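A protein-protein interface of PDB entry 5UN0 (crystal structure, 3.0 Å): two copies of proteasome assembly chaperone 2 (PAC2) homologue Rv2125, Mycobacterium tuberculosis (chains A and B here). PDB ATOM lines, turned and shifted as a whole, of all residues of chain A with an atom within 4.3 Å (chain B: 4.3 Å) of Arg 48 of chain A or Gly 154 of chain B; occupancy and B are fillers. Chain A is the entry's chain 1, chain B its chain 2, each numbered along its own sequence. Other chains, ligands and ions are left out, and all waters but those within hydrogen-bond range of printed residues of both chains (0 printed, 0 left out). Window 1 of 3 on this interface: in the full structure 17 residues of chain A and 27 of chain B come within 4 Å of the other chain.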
ATOM      1  N   TYR A  44       5.398  30.558 -15.822  1.00  0.00           N
ATOM      2  CA  TYR A  44       5.111  29.720 -16.974  1.00  0.00           C
ATOM      3  C   TYR A  44       4.330  30.406 -18.087  1.00  0.00           C
ATOM      4  O   TYR A  44       4.174  29.846 -19.157  1.00  0.00           O
ATOM      5  CB  TYR A  44       4.396  28.469 -16.517  1.00  0.00           C
ATOM      6  CG  TYR A  44       5.267  27.559 -15.688  1.00  0.00           C
ATOM      7  CD1 TYR A  44       6.429  27.026 -16.212  1.00  0.00           C
ATOM      8  CD2 TYR A  44       4.917  27.214 -14.387  1.00  0.00           C
ATOM      9  CE1 TYR A  44       7.234  26.189 -15.465  1.00  0.00           C
ATOM     10  CE2 TYR A  44       5.718  26.365 -13.625  1.00  0.00           C
ATOM     11  CZ  TYR A  44       6.880  25.852 -14.169  1.00  0.00           C
ATOM     12  OH  TYR A  44       7.703  25.008 -13.446  1.00  0.00           O
ATOM     13  N   GLN A  45       3.842  31.620 -17.858  1.00  0.00           N
ATOM     14  CA  GLN A  45       3.319  32.411 -18.965  1.00  0.00           C
ATOM     15  C   GLN A  45       4.481  33.021 -19.735  1.00  0.00           C
ATOM     16  O   GLN A  45       4.378  33.240 -20.940  1.00  0.00           O
ATOM     17  CB  GLN A  45       2.379  33.502 -18.473  1.00  0.00           C
ATOM     18  CG  GLN A  45       0.931  33.065 -18.376  1.00  0.00           C
ATOM     19  CD  GLN A  45       0.034  34.136 -17.790  1.00  0.00           C
ATOM     20  OE1 GLN A  45       0.406  35.298 -17.705  1.00  0.00           O
ATOM     21  NE2 GLN A  45      -1.163  33.745 -17.384  1.00  0.00           N
ATOM     22  N   VAL A  46       5.589  33.285 -19.047  1.00  0.00           N
ATOM     23  CA  VAL A  46       6.746  33.888 -19.675  1.00  0.00           C
ATOM     24  C   VAL A  46       7.509  32.820 -20.385  1.00  0.00           C
ATOM     25  O   VAL A  46       7.710  32.901 -21.600  1.00  0.00           O
ATOM     26  CB  VAL A  46       7.660  34.535 -18.652  1.00  0.00           C
ATOM     27  CG1 VAL A  46       8.894  35.104 -19.329  1.00  0.00           C
ATOM     28  CG2 VAL A  46       6.912  35.635 -17.914  1.00  0.00           C
ATOM     29  N   ASN A  47       7.929  31.814 -19.621  1.00  0.00           N
ATOM     30  CA  ASN A  47       8.551  30.606 -20.171  1.00  0.00           C
ATOM     31  C   ASN A  47       7.543  29.481 -20.285  1.00  0.00           C
ATOM     32  O   ASN A  47       7.396  28.671 -19.346  1.00  0.00           O
ATOM     33  CB  ASN A  47       9.673  30.102 -19.256  1.00  0.00           C
ATOM     34  CG  ASN A  47      10.816  31.070 -19.131  1.00  0.00           C
ATOM     35  OD1 ASN A  47      11.358  31.240 -18.042  1.00  0.00           O
ATOM     36  ND2 ASN A  47      11.216  31.690 -20.237  1.00  0.00           N
ATOM     37  N   ARG A  48       6.853  29.414 -21.419  1.00  0.00           N
ATOM     38  CA  ARG A  48       5.803  28.403 -21.596  1.00  0.00           C
ATOM     39  C   ARG A  48       6.383  26.995 -21.789  1.00  0.00           C
ATOM     40  O   ARG A  48       7.518  26.852 -22.240  1.00  0.00           O
ATOM     41  CB  ARG A  48       4.882  28.785 -22.750  1.00  0.00           C
ATOM     42  CG  ARG A  48       4.101  30.057 -22.465  1.00  0.00           C
ATOM     43  CD  ARG A  48       2.974  30.300 -23.463  1.00  0.00           C
ATOM     44  NE  ARG A  48       2.083  31.364 -22.990  1.00  0.00           N
ATOM     45  CZ  ARG A  48       1.028  31.196 -22.196  1.00  0.00           C
ATOM     46  NH1 ARG A  48       0.323  32.253 -21.819  1.00  0.00           N
ATOM     47  NH2 ARG A  48       0.665  29.990 -21.776  1.00  0.00           N
ATOM     48  N   PRO A  49       5.628  25.953 -21.403  1.00  0.00           N
ATOM     49  CA  PRO A  49       6.115  24.629 -21.724  1.00  0.00           C
ATOM     50  C   PRO A  49       5.803  24.328 -23.157  1.00  0.00           C
ATOM     51  O   PRO A  49       4.955  24.988 -23.764  1.00  0.00           O
ATOM     52  CB  PRO A  49       5.323  23.695 -20.789  1.00  0.00           C
ATOM     53  CG  PRO A  49       4.726  24.588 -19.766  1.00  0.00           C
ATOM     54  CD  PRO A  49       4.483  25.888 -20.488  1.00  0.00           C
ATOM     55  N   VAL A  50       6.499  23.330 -23.682  1.00  0.00           N
ATOM     56  CA  VAL A  50       6.350  22.933 -25.072  1.00  0.00           C
ATOM     57  C   VAL A  50       5.563  21.639 -25.129  1.00  0.00           C
ATOM     58  O   VAL A  50       5.932  20.647 -24.488  1.00  0.00           O
ATOM     59  CB  VAL A  50       7.712  22.758 -25.771  1.00  0.00           C
ATOM     60  CG1 VAL A  50       7.521  22.601 -27.270  1.00  0.00           C
ATOM     61  CG2 VAL A  50       8.615  23.954 -25.504  1.00  0.00           C
ATOM     62  N   TRP B  10      -4.437  34.010 -22.703  1.00  0.00           N
ATOM     63  CA  TRP B  10      -3.732  33.309 -23.783  1.00  0.00           C
ATOM     64  C   TRP B  10      -4.614  32.242 -24.439  1.00  0.00           C
ATOM     65  O   TRP B  10      -4.783  32.232 -25.656  1.00  0.00           O
ATOM     66  CB  TRP B  10      -2.475  32.645 -23.238  1.00  0.00           C
ATOM     67  CG  TRP B  10      -1.465  32.280 -24.281  1.00  0.00           C
ATOM     68  CD1 TRP B  10      -0.630  33.131 -24.943  1.00  0.00           C
ATOM     69  CD2 TRP B  10      -1.136  30.961 -24.746  1.00  0.00           C
ATOM     70  NE1 TRP B  10       0.187  32.433 -25.796  1.00  0.00           N
ATOM     71  CE2 TRP B  10      -0.106  31.101 -25.699  1.00  0.00           C
ATOM     72  CE3 TRP B  10      -1.610  29.671 -24.446  1.00  0.00           C
ATOM     73  CZ2 TRP B  10       0.449  30.010 -26.362  1.00  0.00           C
ATOM     74  CZ3 TRP B  10      -1.058  28.586 -25.118  1.00  0.00           C
ATOM     75  CH2 TRP B  10      -0.041  28.764 -26.058  1.00  0.00           C
ATOM     76  N   ASN B  11      -5.239  31.398 -23.642  1.00  0.00           N
ATOM     77  CA  ASN B  11      -6.017  30.292 -24.132  1.00  0.00           C
ATOM     78  C   ASN B  11      -7.381  30.674 -24.663  1.00  0.00           C
ATOM     79  O   ASN B  11      -8.093  29.832 -25.106  1.00  0.00           O
ATOM     80  CB  ASN B  11      -6.191  29.186 -23.078  1.00  0.00           C
ATOM     81  CG  ASN B  11      -4.916  28.809 -22.367  1.00  0.00           C
ATOM     82  OD1 ASN B  11      -4.167  27.981 -22.806  1.00  0.00           O
ATOM     83  ND2 ASN B  11      -4.710  29.388 -21.249  1.00  0.00           N
ATOM     84  N   GLU B  87      -5.605  32.319 -16.460  1.00  0.00           N
ATOM     85  CA  GLU B  87      -4.517  31.363 -16.481  1.00  0.00           C
ATOM     86  C   GLU B  87      -3.462  31.761 -15.462  1.00  0.00           C
ATOM     87  O   GLU B  87      -2.854  32.810 -15.594  1.00  0.00           O
ATOM     88  CB  GLU B  87      -3.916  31.315 -17.895  1.00  0.00           C
ATOM     89  CG  GLU B  87      -2.651  30.488 -18.033  1.00  0.00           C
ATOM     90  CD  GLU B  87      -2.050  30.629 -19.406  1.00  0.00           C
ATOM     91  OE1 GLU B  87      -1.810  31.756 -19.839  1.00  0.00           O
ATOM     92  OE2 GLU B  87      -1.825  29.606 -20.052  1.00  0.00           O
ATOM     93  N   TRP B  92       1.902  25.815 -11.908  1.00  0.00           N
ATOM     94  CA  TRP B  92       0.980  25.059 -12.749  1.00  0.00           C
ATOM     95  C   TRP B  92       0.831  23.608 -12.294  1.00  0.00           C
ATOM     96  O   TRP B  92      -0.271  23.108 -12.145  1.00  0.00           O
ATOM     97  CB  TRP B  92       1.467  25.087 -14.207  1.00  0.00           C
ATOM     98  CG  TRP B  92       1.243  26.379 -14.913  1.00  0.00           C
ATOM     99  CD1 TRP B  92       0.940  27.563 -14.350  1.00  0.00           C
ATOM    100  CD2 TRP B  92       1.322  26.613 -16.323  1.00  0.00           C
ATOM    101  NE1 TRP B  92       0.790  28.529 -15.313  1.00  0.00           N
ATOM    102  CE2 TRP B  92       1.037  27.970 -16.535  1.00  0.00           C
ATOM    103  CE3 TRP B  92       1.613  25.811 -17.421  1.00  0.00           C
ATOM    104  CZ2 TRP B  92       1.034  28.549 -17.801  1.00  0.00           C
ATOM    105  CZ3 TRP B  92       1.607  26.383 -18.684  1.00  0.00           C
ATOM    106  CH2 TRP B  92       1.313  27.738 -18.865  1.00  0.00           C
ATOM    107  N   PRO B 152       4.829  26.008 -27.830  1.00  0.00           N
ATOM    108  CA  PRO B 152       4.428  26.407 -26.494  1.00  0.00           C
ATOM    109  C   PRO B 152       2.969  26.112 -26.210  1.00  0.00           C
ATOM    110  O   PRO B 152       2.149  26.305 -27.092  1.00  0.00           O
ATOM    111  CB  PRO B 152       4.626  27.928 -26.518  1.00  0.00           C
ATOM    112  CG  PRO B 152       4.484  28.306 -27.948  1.00  0.00           C
ATOM    113  CD  PRO B 152       5.186  27.182 -28.644  1.00  0.00           C
ATOM    114  N   THR B 153       2.655  25.647 -24.996  1.00  0.00           N
ATOM    115  CA  THR B 153       1.266  25.403 -24.580  1.00  0.00           C
ATOM    116  C   THR B 153       0.834  26.344 -23.459  1.00  0.00           C
ATOM    117  O   THR B 153       1.627  27.138 -22.958  1.00  0.00           O
ATOM    118  CB  THR B 153       1.045  23.944 -24.123  1.00  0.00           C
ATOM    119  OG1 THR B 153      -0.356  23.620 -24.180  1.00  0.00           O
ATOM    120  CG2 THR B 153       1.545  23.702 -22.698  1.00  0.00           C
ATOM    121  N   GLY B 154      -0.441  26.261 -23.095  1.00  0.00           N
ATOM    122  CA  GLY B 154      -0.987  26.996 -21.958  1.00  0.00           C
ATOM    123  C   GLY B 154      -1.503  26.022 -20.919  1.00  0.00           C
ATOM    124  O   GLY B 154      -1.262  24.805 -21.017  1.00  0.00           O
ATOM    125  N   ILE B 155      -2.191  26.560 -19.918  1.00  0.00           N
ATOM    126  CA  ILE B 155      -2.723  25.770 -18.813  1.00  0.00           C
ATOM    127  C   ILE B 155      -3.779  24.763 -19.288  1.00  0.00           C
ATOM    128  O   ILE B 155      -3.932  23.671 -18.718  1.00  0.00           O
ATOM    129  CB  ILE B 155      -3.299  26.691 -17.721  1.00  0.00           C
ATOM    130  CG1 ILE B 155      -3.644  25.913 -16.447  1.00  0.00           C
ATOM    131  CG2 ILE B 155      -4.529  27.433 -18.229  1.00  0.00           C
ATOM    132  CD1 ILE B 155      -2.462  25.216 -15.810  1.00  0.00           C
ATOM    133  N   ALA B 156      -4.500  25.137 -20.340  1.00  0.00           N
ATOM    134  CA  ALA B 156      -5.480  24.239 -20.942  1.00  0.00           C
ATOM    135  C   ALA B 156      -4.823  22.890 -21.277  1.00  0.00           C
ATOM    136  O   ALA B 156      -5.219  21.850 -20.766  1.00  0.00           O
ATOM    137  CB  ALA B 156      -6.100  24.872 -22.183  1.00  0.00           C
ATOM    138  N   GLY B 157      -3.799  22.930 -22.109  1.00  0.00           N
ATOM    139  CA  GLY B 157      -3.110  21.723 -22.549  1.00  0.00           C
ATOM    140  C   GLY B 157      -2.429  20.964 -21.431  1.00  0.00           C
ATOM    141  O   GLY B 157      -2.375  19.742 -21.448  1.00  0.00           O
ATOM    142  N   VAL B 158      -1.894  21.693 -20.462  1.00  0.00           N
ATOM    143  CA  VAL B 158      -1.219  21.071 -19.321  1.00  0.00           C
ATOM    144  C   VAL B 158      -2.231  20.310 -18.479  1.00  0.00           C
ATOM    145  O   VAL B 158      -2.041  19.151 -18.134  1.00  0.00           O
ATOM    146  CB  VAL B 158      -0.520  22.134 -18.443  1.00  0.00           C
ATOM    147  CG1 VAL B 158       0.001  21.531 -17.147  1.00  0.00           C
ATOM    148  CG2 VAL B 158       0.625  22.748 -19.212  1.00  0.00           C
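Of the 11 printed residues of chain B, 6 touch a printed residue of chain A.
Of the 7 printed residues of chain A, 4 touch a printed residue of chain B.
Among the printed residues, 11 pairs touch across the chains.
Among the printed residues, Asp or Glu carboxylates within 4 Å of a Lys or Arg side-chain nitrogen of the other chain: Arg 48 of chain A with Glu 87 of chain B.
No position is printed for both chains.
Of chain B, only Trp 10 (3.0 Å), Glu 87 (3.0 Å), Trp 92 (3.7 Å), Pro 152 (3.9 Å), Thr 153 (3.2 Å) and Gly 154 (3.4 Å) come within 4 Å of Arg 48 of chain A.
Gly 154 of chain B touches just one residue of chain A: Arg 48 (3.4 Å).
Printed residues of chain A within 4 Å of Pro 152 of chain B: Arg 48 and Pro 49.
Of the printed residues of chain A, Thr 153 of chain B touches Arg 48 and Pro 49.
Of the printed residues of chain A, Glu 87 of chain B touches Gln 45 (2.6 Å) and Arg 48 (3.0 Å).
Ile 155 of chain B touches none of the printed residues of chain A.
The nearest printed residue of chain B that does not touch Arg 48 of chain A is Ile 155 of chain B (4.8 Å).
The nearest printed residue of chain B that does not touch Tyr 44 of chain A is Thr 153 of chain B (5.3 Å).
Among the printed residues, pairs that only touch across the chains: Tyr 44 of chain A with Trp 92 of chain B (3.4 Å), Arg 48 of chain A with Trp 10 of chain B (3.0 Å), Arg 48 of chain A with Trp 92 of chain B (3.7 Å), Arg 48 of chain A with Pro 152 of chain B (3.9 Å), Arg 48 of chain A with Gly 154 of chain B (3.4 Å), Pro 49 of chain A with Trp 92 of chain B (3.4 Å) and Pro 49 of chain A with Pro 152 of chain B (3.1 Å).
The backbone carbonyl oxygen (O) of Thr 153 of chain B is in hydrogen-bond range of the guanidinium group (NH2) of Arg 48 of chain A (3.2 Å).
O of Pro 49 of chain A sits at hydrogen-bond distance from N of Thr 153 of chain B, at 2.7 Å.
NH1 of Arg 48 of chain A is in salt-bridge range of OE1 of Glu 87 of chain B, at 3.0 Å.
The side-chain amide nitrogen (NE2) of Gln 45 of chain A lies within hydrogen-bond range of the backbone carbonyl oxygen (O) of Glu 87 of chain B.
OE2 of Glu 87 of chain B sits at hydrogen-bond distance from ND2 of Asn 11 of chain B (3.1 Å).
The backbone NH (N) of Ile 155 of chain B sits at hydrogen-bond distance from the side-chain carboxylate (OE2) of Glu 87 of chain B (3.1 Å).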
